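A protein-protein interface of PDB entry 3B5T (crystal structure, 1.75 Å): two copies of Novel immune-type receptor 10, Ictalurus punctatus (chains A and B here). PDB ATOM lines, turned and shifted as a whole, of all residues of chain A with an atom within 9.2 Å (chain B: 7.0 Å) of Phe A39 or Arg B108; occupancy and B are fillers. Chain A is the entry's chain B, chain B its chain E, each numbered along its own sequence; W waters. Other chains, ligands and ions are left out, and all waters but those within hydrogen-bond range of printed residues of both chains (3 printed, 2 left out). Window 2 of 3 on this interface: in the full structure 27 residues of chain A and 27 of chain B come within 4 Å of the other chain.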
ATOM      1  N   ARG A  36      -6.589  -9.882  23.217  1.00  0.00           N
ATOM      2  CA  ARG A  36      -5.785  -8.727  22.850  1.00  0.00           C
ATOM      3  C   ARG A  36      -6.125  -8.291  21.424  1.00  0.00           C
ATOM      4  O   ARG A  36      -6.140  -9.123  20.522  1.00  0.00           O
ATOM      5  CB  ARG A  36      -4.299  -9.088  22.891  1.00  0.00           C
ATOM      6  CG  ARG A  36      -3.419  -7.913  22.563  1.00  0.00           C
ATOM      7  CD  ARG A  36      -1.970  -8.294  22.793  1.00  0.00           C
ATOM      8  NE  ARG A  36      -1.074  -7.294  22.246  1.00  0.00           N
ATOM      9  CZ  ARG A  36       0.241  -7.442  22.222  1.00  0.00           C
ATOM     10  NH1 ARG A  36       0.782  -8.549  22.723  1.00  0.00           N
ATOM     11  NH2 ARG A  36       1.000  -6.492  21.710  1.00  0.00           N
ATOM     12  N   GLN A  37      -6.418  -7.012  21.259  1.00  0.00           N
ATOM     13  CA  GLN A  37      -6.678  -6.444  19.945  1.00  0.00           C
ATOM     14  C   GLN A  37      -5.717  -5.291  19.617  1.00  0.00           C
ATOM     15  O   GLN A  37      -5.830  -4.182  20.137  1.00  0.00           O
ATOM     16  CB  GLN A  37      -8.142  -6.005  19.812  1.00  0.00           C
ATOM     17  CG  GLN A  37      -8.427  -5.444  18.403  1.00  0.00           C
ATOM     18  CD  GLN A  37      -9.643  -4.557  18.323  1.00  0.00           C
ATOM     19  OE1 GLN A  37     -10.174  -4.068  19.342  1.00  0.00           O
ATOM     20  NE2 GLN A  37     -10.102  -4.328  17.093  1.00  0.00           N
ATOM     21  N   SER A  38      -4.751  -5.572  18.755  1.00  0.00           N
ATOM     22  CA  SER A  38      -3.897  -4.522  18.204  1.00  0.00           C
ATOM     23  C   SER A  38      -4.773  -3.610  17.316  1.00  0.00           C
ATOM     24  O   SER A  38      -5.759  -4.081  16.743  1.00  0.00           O
ATOM     25  CB  SER A  38      -2.757  -5.154  17.405  1.00  0.00           C
ATOM     26  OG  SER A  38      -1.903  -5.875  18.282  1.00  0.00           O
ATOM     27  N   PHE A  39      -4.452  -2.320  17.230  1.00  0.00           N
ATOM     28  CA  PHE A  39      -5.297  -1.417  16.455  1.00  0.00           C
ATOM     29  C   PHE A  39      -5.412  -1.880  15.005  1.00  0.00           C
ATOM     30  O   PHE A  39      -4.426  -2.280  14.391  1.00  0.00           O
ATOM     31  CB  PHE A  39      -4.829   0.036  16.527  1.00  0.00           C
ATOM     32  CG  PHE A  39      -5.792   1.002  15.878  1.00  0.00           C
ATOM     33  CD1 PHE A  39      -6.846   1.556  16.609  1.00  0.00           C
ATOM     34  CD2 PHE A  39      -5.661   1.341  14.530  1.00  0.00           C
ATOM     35  CE1 PHE A  39      -7.737   2.435  16.014  1.00  0.00           C
ATOM     36  CE2 PHE A  39      -6.554   2.227  13.925  1.00  0.00           C
ATOM     37  CZ  PHE A  39      -7.589   2.777  14.668  1.00  0.00           C
ATOM     38  N   GLY A  40      -6.641  -1.850  14.490  1.00  0.00           N
ATOM     39  CA  GLY A  40      -6.931  -2.299  13.132  1.00  0.00           C
ATOM     40  C   GLY A  40      -6.860  -3.785  12.855  1.00  0.00           C
ATOM     41  O   GLY A  40      -6.932  -4.187  11.701  1.00  0.00           O
ATOM     42  N   LYS A  41      -6.746  -4.601  13.909  1.00  0.00           N
ATOM     43  CA  LYS A  41      -6.738  -6.073  13.797  1.00  0.00           C
ATOM     44  C   LYS A  41      -7.944  -6.710  14.485  1.00  0.00           C
ATOM     45  O   LYS A  41      -8.554  -6.096  15.346  1.00  0.00           O
ATOM     46  CB  LYS A  41      -5.478  -6.676  14.448  1.00  0.00           C
ATOM     47  CG  LYS A  41      -4.134  -6.121  13.975  1.00  0.00           C
ATOM     48  CD  LYS A  41      -3.947  -6.221  12.475  1.00  0.00           C
ATOM     49  CE  LYS A  41      -2.591  -5.641  12.081  1.00  0.00           C
ATOM     50  NZ  LYS A  41      -1.984  -6.519  11.052  1.00  0.00           N
ATOM     51  N   VAL A  42      -8.240  -7.959  14.124  1.00  0.00           N
ATOM     52  CA  VAL A  42      -9.243  -8.761  14.801  1.00  0.00           C
ATOM     53  C   VAL A  42      -8.692  -9.134  16.194  1.00  0.00           C
ATOM     54  O   VAL A  42      -7.495  -9.418  16.322  1.00  0.00           O
ATOM     55  CB  VAL A  42      -9.550 -10.016  13.952  1.00  0.00           C
ATOM     56  CG1 VAL A  42     -10.516 -10.906  14.624  1.00  0.00           C
ATOM     57  CG2 VAL A  42     -10.094  -9.602  12.550  1.00  0.00           C
ATOM     58  N   PRO A  43      -9.532  -9.069  17.251  1.00  0.00           N
ATOM     59  CA  PRO A  43      -9.045  -9.490  18.570  1.00  0.00           C
ATOM     60  C   PRO A  43      -8.595 -10.949  18.557  1.00  0.00           C
ATOM     61  O   PRO A  43      -9.154 -11.780  17.810  1.00  0.00           O
ATOM     62  CB  PRO A  43     -10.289  -9.356  19.462  1.00  0.00           C
ATOM     63  CG  PRO A  43     -11.166  -8.343  18.755  1.00  0.00           C
ATOM     64  CD  PRO A  43     -10.932  -8.598  17.299  1.00  0.00           C
ATOM     65  N   GLU A  85       5.351   0.918  23.106  1.00  0.00           N
ATOM     66  CA  GLU A  85       4.394   1.305  22.084  1.00  0.00           C
ATOM     67  C   GLU A  85       3.656   0.121  21.449  1.00  0.00           C
ATOM     68  O   GLU A  85       2.449   0.206  21.225  1.00  0.00           O
ATOM     69  CB  GLU A  85       5.095   2.169  21.029  1.00  0.00           C
ATOM     70  CG  GLU A  85       5.348   3.624  21.473  1.00  0.00           C
ATOM     71  CD  GLU A  85       6.488   3.803  22.494  1.00  0.00           C
ATOM     72  OE1 GLU A  85       7.204   2.826  22.825  1.00  0.00           O
ATOM     73  OE2 GLU A  85       6.661   4.947  22.975  1.00  0.00           O
ATOM     74  N   ASP A  86       4.388  -0.969  21.206  1.00  0.00           N
ATOM     75  CA  ASP A  86       3.866  -2.206  20.598  1.00  0.00           C
ATOM     76  C   ASP A  86       2.725  -2.826  21.396  1.00  0.00           C
ATOM     77  O   ASP A  86       1.894  -3.554  20.835  1.00  0.00           O
ATOM     78  CB  ASP A  86       4.972  -3.265  20.495  1.00  0.00           C
ATOM     79  CG  ASP A  86       5.832  -3.124  19.235  1.00  0.00           C
ATOM     80  OD1 ASP A  86       5.447  -2.399  18.286  1.00  0.00           O
ATOM     81  OD2 ASP A  86       6.914  -3.756  19.204  1.00  0.00           O
ATOM     82  N   ASP A  87       2.731  -2.588  22.710  1.00  0.00           N
ATOM     83  CA  ASP A  87       1.721  -3.137  23.622  1.00  0.00           C
ATOM     84  C   ASP A  87       0.378  -2.456  23.476  1.00  0.00           C
ATOM     85  O   ASP A  87      -0.654  -2.981  23.951  1.00  0.00           O
ATOM     86  CB  ASP A  87       2.166  -2.965  25.082  1.00  0.00           C
ATOM     87  CG  ASP A  87       3.414  -3.740  25.424  1.00  0.00           C
ATOM     88  OD1 ASP A  87       3.700  -4.792  24.807  1.00  0.00           O
ATOM     89  OD2 ASP A  87       4.118  -3.302  26.358  1.00  0.00           O
ATOM     90  N   GLY A  88       0.391  -1.275  22.860  1.00  0.00           N
ATOM     91  CA  GLY A  88      -0.804  -0.462  22.718  1.00  0.00           C
ATOM     92  C   GLY A  88      -1.934  -1.236  22.058  1.00  0.00           C
ATOM     93  O   GLY A  88      -1.705  -2.067  21.189  1.00  0.00           O
ATOM     94  N   GLY A  89      -3.159  -0.972  22.499  1.00  0.00           N
ATOM     95  CA  GLY A  89      -4.322  -1.626  21.894  1.00  0.00           C
ATOM     96  C   GLY A  89      -5.431  -1.762  22.909  1.00  0.00           C
ATOM     97  O   GLY A  89      -5.452  -1.053  23.907  1.00  0.00           O
ATOM     98  N   GLU A  90      -6.365  -2.664  22.638  1.00  0.00           N
ATOM     99  CA  GLU A  90      -7.473  -2.899  23.545  1.00  0.00           C
ATOM    100  C   GLU A  90      -7.456  -4.346  24.018  1.00  0.00           C
ATOM    101  O   GLU A  90      -7.153  -5.267  23.261  1.00  0.00           O
ATOM    102  CB  GLU A  90      -8.803  -2.507  22.881  1.00  0.00           C
ATOM    103  CG  GLU A  90      -8.842  -0.995  22.594  1.00  0.00           C
ATOM    104  CD  GLU A  90     -10.118  -0.502  21.966  1.00  0.00           C
ATOM    105  OE1 GLU A  90     -10.992  -1.327  21.633  1.00  0.00           O
ATOM    106  OE2 GLU A  90     -10.221   0.734  21.805  1.00  0.00           O
ATOM    107  N   TYR A  91      -7.761  -4.537  25.294  1.00  0.00           N
ATOM    108  CA  TYR A  91      -7.684  -5.849  25.908  1.00  0.00           C
ATOM    109  C   TYR A  91      -9.032  -6.074  26.556  1.00  0.00           C
ATOM    110  O   TYR A  91      -9.534  -5.182  27.249  1.00  0.00           O
ATOM    111  CB  TYR A  91      -6.597  -5.884  26.991  1.00  0.00           C
ATOM    112  CG  TYR A  91      -5.187  -5.749  26.436  1.00  0.00           C
ATOM    113  CD1 TYR A  91      -4.376  -6.864  26.282  1.00  0.00           C
ATOM    114  CD2 TYR A  91      -4.689  -4.494  26.038  1.00  0.00           C
ATOM    115  CE1 TYR A  91      -3.083  -6.738  25.756  1.00  0.00           C
ATOM    116  CE2 TYR A  91      -3.407  -4.360  25.517  1.00  0.00           C
ATOM    117  CZ  TYR A  91      -2.614  -5.486  25.395  1.00  0.00           C
ATOM    118  OH  TYR A  91      -1.348  -5.382  24.880  1.00  0.00           O
ATOM    119  N   ARG A 108      -8.289   0.055  27.262  1.00  0.00           N
ATOM    120  CA  ARG A 108      -7.513   0.589  26.151  1.00  0.00           C
ATOM    121  C   ARG A 108      -6.189   1.095  26.718  1.00  0.00           C
ATOM    122  O   ARG A 108      -6.157   1.966  27.592  1.00  0.00           O
ATOM    123  CB  ARG A 108      -8.246   1.717  25.431  1.00  0.00           C
ATOM    124  CG  ARG A 108      -7.435   2.298  24.267  1.00  0.00           C
ATOM    125  CD  ARG A 108      -8.147   3.494  23.638  1.00  0.00           C
ATOM    126  NE  ARG A 108      -9.500   3.118  23.211  1.00  0.00           N
ATOM    127  CZ  ARG A 108     -10.501   3.967  22.997  1.00  0.00           C
ATOM    128  NH1 ARG A 108     -10.333   5.282  23.150  1.00  0.00           N
ATOM    129  NH2 ARG A 108     -11.680   3.494  22.617  1.00  0.00           N
ATOM    130  N   LEU A 109      -5.114   0.527  26.214  1.00  0.00           N
ATOM    131  CA  LEU A 109      -3.785   0.910  26.624  1.00  0.00           C
ATOM    132  C   LEU A 109      -3.234   1.793  25.510  1.00  0.00           C
ATOM    133  O   LEU A 109      -3.167   1.371  24.359  1.00  0.00           O
ATOM    134  CB  LEU A 109      -2.941  -0.349  26.817  1.00  0.00           C
ATOM    135  CG  LEU A 109      -1.562  -0.216  27.462  1.00  0.00           C
ATOM    136  CD1 LEU A 109      -1.680   0.438  28.827  1.00  0.00           C
ATOM    137  CD2 LEU A 109      -0.890  -1.579  27.558  1.00  0.00           C
ATOM    138  N   GLN A 110      -2.848   3.017  25.865  1.00  0.00           N
ATOM    139  CA  GLN A 110      -2.411   4.000  24.877  1.00  0.00           C
ATOM    140  C   GLN A 110      -1.239   4.851  25.379  1.00  0.00           C
ATOM    141  O   GLN A 110      -0.989   4.949  26.592  1.00  0.00           O
ATOM    142  CB  GLN A 110      -3.580   4.892  24.451  1.00  0.00           C
ATOM    143  CG  GLN A 110      -4.164   5.716  25.569  1.00  0.00           C
ATOM    144  CD  GLN A 110      -5.307   6.585  25.122  1.00  0.00           C
ATOM    145  OE1 GLN A 110      -6.034   6.243  24.183  1.00  0.00           O
ATOM    146  NE2 GLN A 110      -5.491   7.709  25.800  1.00  0.00           N
ATOM    147  N   GLU B   5      -6.612  -8.534   9.558  1.00  0.00           N
ATOM    148  CA  GLU B   5      -6.864  -7.108   9.577  1.00  0.00           C
ATOM    149  C   GLU B   5      -8.363  -6.890   9.572  1.00  0.00           C
ATOM    150  O   GLU B   5      -9.094  -7.616   8.895  1.00  0.00           O
ATOM    151  CB  GLU B   5      -6.291  -6.447   8.321  1.00  0.00           C
ATOM    152  CG  GLU B   5      -4.809  -6.666   8.101  1.00  0.00           C
ATOM    153  CD  GLU B   5      -3.966  -5.606   8.768  1.00  0.00           C
ATOM    154  OE1 GLU B   5      -4.537  -4.691   9.400  1.00  0.00           O
ATOM    155  OE2 GLU B   5      -2.722  -5.681   8.653  1.00  0.00           O
ATOM    156  N   LEU B   6      -8.819  -5.883  10.304  1.00  0.00           N
ATOM    157  CA  LEU B   6     -10.200  -5.442  10.141  1.00  0.00           C
ATOM    158  C   LEU B   6     -10.372  -4.782   8.784  1.00  0.00           C
ATOM    159  O   LEU B   6      -9.498  -4.029   8.327  1.00  0.00           O
ATOM    160  CB  LEU B   6     -10.578  -4.401  11.180  1.00  0.00           C
ATOM    161  CG  LEU B   6     -10.534  -4.742  12.657  1.00  0.00           C
ATOM    162  CD1 LEU B   6     -10.757  -3.467  13.468  1.00  0.00           C
ATOM    163  CD2 LEU B   6     -11.581  -5.810  12.951  1.00  0.00           C
ATOM    164  N   HIS B   7     -11.515  -5.031   8.166  1.00  0.00           N
ATOM    165  CA  HIS B   7     -11.964  -4.191   7.075  1.00  0.00           C
ATOM    166  C   HIS B   7     -12.329  -2.819   7.645  1.00  0.00           C
ATOM    167  O   HIS B   7     -13.073  -2.733   8.633  1.00  0.00           O
ATOM    168  CB  HIS B   7     -13.160  -4.804   6.363  1.00  0.00           C
ATOM    169  CG  HIS B   7     -13.569  -4.043   5.141  1.00  0.00           C
ATOM    170  ND1 HIS B   7     -14.809  -3.457   5.006  1.00  0.00           N
ATOM    171  CD2 HIS B   7     -12.890  -3.754   4.003  1.00  0.00           C
ATOM    172  CE1 HIS B   7     -14.876  -2.842   3.836  1.00  0.00           C
ATOM    173  NE2 HIS B   7     -13.727  -3.008   3.209  1.00  0.00           N
ATOM    174  N   VAL B   8     -11.781  -1.757   7.061  1.00  0.00           N
ATOM    175  CA  VAL B   8     -12.089  -0.385   7.495  1.00  0.00           C
ATOM    176  C   VAL B   8     -13.080   0.221   6.510  1.00  0.00           C
ATOM    177  O   VAL B   8     -12.835   0.258   5.313  1.00  0.00           O
ATOM    178  CB  VAL B   8     -10.816   0.513   7.549  1.00  0.00           C
ATOM    179  CG1 VAL B   8     -11.150   1.943   7.981  1.00  0.00           C
ATOM    180  CG2 VAL B   8      -9.777  -0.097   8.468  1.00  0.00           C
ATOM    181  N   LYS B   9     -14.209   0.685   7.019  1.00  0.00           N
ATOM    182  CA  LYS B   9     -15.221   1.278   6.169  1.00  0.00           C
ATOM    183  C   LYS B   9     -15.597   2.651   6.717  1.00  0.00           C
ATOM    184  O   LYS B   9     -15.987   2.780   7.884  1.00  0.00           O
ATOM    185  CB  LYS B   9     -16.431   0.350   6.144  1.00  0.00           C
ATOM    186  CG  LYS B   9     -17.545   0.803   5.263  1.00  0.00           C
ATOM    187  CD  LYS B   9     -18.545  -0.347   5.082  1.00  0.00           C
ATOM    188  CE  LYS B   9     -19.533  -0.010   3.989  1.00  0.00           C
ATOM    189  NZ  LYS B   9     -18.905  -0.018   2.639  1.00  0.00           N
ATOM    190  N   THR B  10     -15.470   3.674   5.882  1.00  0.00           N
ATOM    191  CA  THR B  10     -15.864   5.023   6.264  1.00  0.00           C
ATOM    192  C   THR B  10     -17.166   5.322   5.541  1.00  0.00           C
ATOM    193  O   THR B  10     -17.239   5.239   4.308  1.00  0.00           O
ATOM    194  CB  THR B  10     -14.791   6.088   5.896  1.00  0.00           C
ATOM    195  OG1 THR B  10     -13.549   5.759   6.551  1.00  0.00           O
ATOM    196  CG2 THR B  10     -15.244   7.475   6.360  1.00  0.00           C
ATOM    197  N   MET B  19     -21.252  -6.220   6.339  1.00  0.00           N
ATOM    198  CA  MET B  19     -19.977  -6.617   6.907  1.00  0.00           C
ATOM    199  C   MET B  19     -19.882  -8.129   6.826  1.00  0.00           C
ATOM    200  O   MET B  19     -20.829  -8.836   7.189  1.00  0.00           O
ATOM    201  CB  MET B  19     -19.925  -6.129   8.348  1.00  0.00           C
ATOM    202  CG  MET B  19     -19.889  -4.610   8.385  1.00  0.00           C
ATOM    203  SD  MET B  19     -19.918  -3.859  10.184  1.00  0.00           S
ATOM    204  CE  MET B  19     -21.839  -3.823  10.469  1.00  0.00           C
ATOM    205  N   PHE B  39     -17.334   2.604  20.112  1.00  0.00           N
ATOM    206  CA  PHE B  39     -16.027   3.156  20.386  1.00  0.00           C
ATOM    207  C   PHE B  39     -15.907   3.497  21.870  1.00  0.00           C
ATOM    208  O   PHE B  39     -16.819   4.093  22.452  1.00  0.00           O
ATOM    209  CB  PHE B  39     -15.775   4.402  19.522  1.00  0.00           C
ATOM    210  CG  PHE B  39     -15.626   4.102  18.046  1.00  0.00           C
ATOM    211  CD1 PHE B  39     -16.448   4.736  17.108  1.00  0.00           C
ATOM    212  CD2 PHE B  39     -14.650   3.219  17.589  1.00  0.00           C
ATOM    213  CE1 PHE B  39     -16.311   4.484  15.734  1.00  0.00           C
ATOM    214  CE2 PHE B  39     -14.494   2.964  16.217  1.00  0.00           C
ATOM    215  CZ  PHE B  39     -15.340   3.601  15.287  1.00  0.00           C
ATOM    216  N   GLY B  88     -21.387   3.481  14.792  1.00  0.00           N
ATOM    217  CA  GLY B  88     -19.938   3.511  14.590  1.00  0.00           C
ATOM    218  C   GLY B  88     -19.283   2.609  15.614  1.00  0.00           C
ATOM    219  O   GLY B  88     -19.718   2.545  16.757  1.00  0.00           O
ATOM    220  N   GLY B  89     -18.239   1.901  15.199  1.00  0.00           N
ATOM    221  CA  GLY B  89     -17.494   1.036  16.123  1.00  0.00           C
ATOM    222  C   GLY B  89     -16.863  -0.101  15.364  1.00  0.00           C
ATOM    223  O   GLY B  89     -16.642  -0.003  14.166  1.00  0.00           O
ATOM    224  N   GLU B  90     -16.556  -1.182  16.072  1.00  0.00           N
ATOM    225  CA  GLU B  90     -15.921  -2.315  15.448  1.00  0.00           C
ATOM    226  C   GLU B  90     -16.797  -3.528  15.673  1.00  0.00           C
ATOM    227  O   GLU B  90     -17.344  -3.716  16.751  1.00  0.00           O
ATOM    228  CB  GLU B  90     -14.511  -2.514  16.010  1.00  0.00           C
ATOM    229  CG  GLU B  90     -13.599  -1.299  15.785  1.00  0.00           C
ATOM    230  CD  GLU B  90     -12.181  -1.511  16.311  1.00  0.00           C
ATOM    231  OE1 GLU B  90     -11.966  -2.413  17.152  1.00  0.00           O
ATOM    232  OE2 GLU B  90     -11.285  -0.783  15.857  1.00  0.00           O
ATOM    233  N   TYR B  91     -16.979  -4.311  14.620  1.00  0.00           N
ATOM    234  CA  TYR B  91     -17.828  -5.488  14.656  1.00  0.00           C
ATOM    235  C   TYR B  91     -16.963  -6.700  14.390  1.00  0.00           C
ATOM    236  O   TYR B  91     -16.168  -6.700  13.419  1.00  0.00           O
ATOM    237  CB  TYR B  91     -18.929  -5.382  13.593  1.00  0.00           C
ATOM    238  CG  TYR B  91     -19.904  -4.240  13.853  1.00  0.00           C
ATOM    239  CD1 TYR B  91     -21.190  -4.507  14.320  1.00  0.00           C
ATOM    240  CD2 TYR B  91     -19.536  -2.897  13.614  1.00  0.00           C
ATOM    241  CE1 TYR B  91     -22.090  -3.475  14.552  1.00  0.00           C
ATOM    242  CE2 TYR B  91     -20.420  -1.849  13.868  1.00  0.00           C
ATOM    243  CZ  TYR B  91     -21.704  -2.157  14.311  1.00  0.00           C
ATOM    244  OH  TYR B  91     -22.582  -1.143  14.583  1.00  0.00           O
ATOM    245  N   PHE B  92     -17.097  -7.711  15.247  1.00  0.00           N
ATOM    246  CA  PHE B  92     -16.252  -8.919  15.158  1.00  0.00           C
ATOM    247  C   PHE B  92     -17.115 -10.164  14.994  1.00  0.00           C
ATOM    248  O   PHE B  92     -18.125 -10.316  15.688  1.00  0.00           O
ATOM    249  CB  PHE B  92     -15.368  -9.096  16.408  1.00  0.00           C
ATOM    250  CG  PHE B  92     -14.707  -7.827  16.896  1.00  0.00           C
ATOM    251  CD1 PHE B  92     -13.855  -7.071  16.069  1.00  0.00           C
ATOM    252  CD2 PHE B  92     -14.906  -7.404  18.209  1.00  0.00           C
ATOM    253  CE1 PHE B  92     -13.235  -5.900  16.547  1.00  0.00           C
ATOM    254  CE2 PHE B  92     -14.305  -6.231  18.683  1.00  0.00           C
ATOM    255  CZ  PHE B  92     -13.471  -5.480  17.865  1.00  0.00           C
ATOM    256  N   GLY B 106     -13.559  -9.055  11.045  1.00  0.00           N
ATOM    257  CA  GLY B 106     -14.176  -7.899  11.687  1.00  0.00           C
ATOM    258  C   GLY B 106     -14.118  -6.677  10.789  1.00  0.00           C
ATOM    259  O   GLY B 106     -13.271  -6.583   9.882  1.00  0.00           O
ATOM    260  N   THR B 107     -15.032  -5.743  11.039  1.00  0.00           N
ATOM    261  CA  THR B 107     -15.070  -4.467  10.308  1.00  0.00           C
ATOM    262  C   THR B 107     -15.105  -3.284  11.245  1.00  0.00           C
ATOM    263  O   THR B 107     -15.843  -3.302  12.232  1.00  0.00           O
ATOM    264  CB  THR B 107     -16.294  -4.414   9.352  1.00  0.00           C
ATOM    265  OG1 THR B 107     -16.145  -5.438   8.374  1.00  0.00           O
ATOM    266  CG2 THR B 107     -16.408  -3.039   8.635  1.00  0.00           C
ATOM    267  N   ARG B 108     -14.306  -2.267  10.939  1.00  0.00           N
ATOM    268  CA  ARG B 108     -14.394  -0.992  11.635  1.00  0.00           C
ATOM    269  C   ARG B 108     -15.304  -0.069  10.827  1.00  0.00           C
ATOM    270  O   ARG B 108     -14.970   0.300   9.687  1.00  0.00           O
ATOM    271  CB  ARG B 108     -13.007  -0.378  11.839  1.00  0.00           C
ATOM    272  CG  ARG B 108     -13.006   0.922  12.662  1.00  0.00           C
ATOM    273  CD  ARG B 108     -11.608   1.204  13.249  1.00  0.00           C
ATOM    274  NE  ARG B 108     -10.828   2.098  12.407  1.00  0.00           N
ATOM    275  CZ  ARG B 108      -9.652   1.816  11.831  1.00  0.00           C
ATOM    276  NH1 ARG B 108      -9.047   0.637  12.003  1.00  0.00           N
ATOM    277  NH2 ARG B 108      -9.062   2.743  11.076  1.00  0.00           N
ATOM    278  N   LEU B 109     -16.444   0.289  11.423  1.00  0.00           N
ATOM    279  CA  LEU B 109     -17.395   1.235  10.823  1.00  0.00           C
ATOM    280  C   LEU B 109     -17.166   2.650  11.397  1.00  0.00           C
ATOM    281  O   LEU B 109     -17.406   2.907  12.583  1.00  0.00           O
ATOM    282  CB  LEU B 109     -18.819   0.744  11.082  1.00  0.00           C
ATOM    283  CG  LEU B 109     -19.979   1.294  10.268  1.00  0.00           C
ATOM    284  CD1 LEU B 109     -19.747   1.132   8.748  1.00  0.00           C
ATOM    285  CD2 LEU B 109     -21.292   0.582  10.685  1.00  0.00           C
ATOM    286  N   GLN B 110     -16.671   3.560  10.560  1.00  0.00           N
ATOM    287  CA  GLN B 110     -16.334   4.898  11.041  1.00  0.00           C
ATOM    288  C   GLN B 110     -17.012   5.997  10.241  1.00  0.00           C
ATOM    289  O   GLN B 110     -17.320   5.825   9.053  1.00  0.00           O
ATOM    290  CB  GLN B 110     -14.819   5.116  11.061  1.00  0.00           C
ATOM    291  CG  GLN B 110     -14.103   4.557   9.878  1.00  0.00           C
ATOM    292  CD  GLN B 110     -12.603   4.753   9.937  1.00  0.00           C
ATOM    293  OE1 GLN B 110     -11.955   4.476  10.954  1.00  0.00           O
ATOM    294  NE2 GLN B 110     -12.037   5.209   8.829  1.00  0.00           N
HETATM  295  O   HOH W   1      -9.639  -0.737  18.447  1.00  0.00           O
HETATM  296  O   HOH W   2      -9.010  -0.314  14.824  1.00  0.00           O
HETATM  297  O   HOH W   3      -3.780  -2.315  11.278  1.00  0.00           O
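NE2 of Gln A37 touches CD1 of Leu B6, 3.8 Å away. Gln A37 touches Phe B92. Phe A39 touches Arg B108 (CE2 to NH1, 3.5 Å). NH1 of Arg B108 touches CA of Gly A40 (3.8 Å). Leu B6 touches Lys A41. Gly B106 touches Val A42. Phe B92 touches Pro A43 (CD1 to CD, 3.5 Å).
Printed residues of chain B within 4 Å of Phe A39: Arg B108 (3.5 Å). Arg B108 touches just these residues of chain A: Phe A39 (3.5 Å) and Gly A40 (3.8 Å). No residue of chain A comes within 4 Å of Val B8. No residue of chain A comes within 4 Å of Thr B107. Printed residues of chain A within 4 Å of Leu B6: Gln A37 (3.8 Å), Gly A40 (2.9 Å) and Lys A41 (3.6 Å). Of the printed residues of chain A, Glu B90 touches Gln A37 (2.7 Å). Of the printed residues of chain A, Glu B5 touches Gly A40 (3.4 Å) and Lys A41 (2.6 Å). His B7 touches none of the printed residues of chain A. The nearest residue of chain B that does not touch Phe A39 is Glu B90 (4.8 Å).
Water W2 lies within hydrogen-bond range of OE2 of Glu B90, N of Gly A40 and NH1 of Arg B108. Water W1 bridges OE2 of Glu B90 (3.1 Å) and OE1 of Gln A37 (3.5 Å). Water W3 lies within hydrogen-bond range of OE1 of Glu B5 and O of Phe A39.
The side-chain amide nitrogen (NE2) of Gln A37 is in hydrogen-bond range of the backbone carbonyl oxygen (O) of Lys A41 (2.9 Å). O of Glu A90 lies within hydrogen-bond range of N of Gln A37, 2.8 Å away. N of His B7 sits at hydrogen-bond distance from O of Gly B106 (2.9 Å). O of His B7 is in hydrogen-bond range of N of Arg B108, at 2.7 Å. The backbone NH of Lys B9 is in hydrogen-bond range of the backbone carbonyl oxygen of Arg B108, at 2.8 Å. The side-chain amide oxygen of Gln B110 lies within hydrogen-bond range of the guanidinium group of Arg B108 (3.0 Å).
Of the 18 printed residues of chain A, 6 touch a printed residue of chain B. Hydrophobic or aromatic side chains of chain A that line the printed part of chain B: Phe A39, Val A42 and Pro A43. Hydrophobic or aromatic side chains of chain B that line the printed part of chain A: Leu B6 and Phe B92. Among the printed residues, 11 pairs touch across the chains.
OE1 of Glu B90 sits at hydrogen-bond distance from NE2 of Gln A37 (2.7 Å). The backbone carbonyl oxygen of Gly A40 lies within hydrogen-bond range of the backbone NH of Leu B6, 2.9 Å away. The side-chain amino group (NZ) of Lys A41 lies within salt-bridge range of the side-chain carboxylate (OE2) of Glu B5, 2.6 Å away. The side-chain carboxylate of Glu B5 sits close to the backbone carbonyl oxygen of Gly A40 (3.4 Å).
Phe A39 touches Arg B108, but with the chains exchanged Arg A108 does not touch Phe B39 (4.3 Å). Positions printed for both chains: 39, 88, 89, 90, 91, 108, 109 and 110. Of the 11 pairs that touch across the chains among the printed residues, none has its exchanged pair printed and touching as well.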
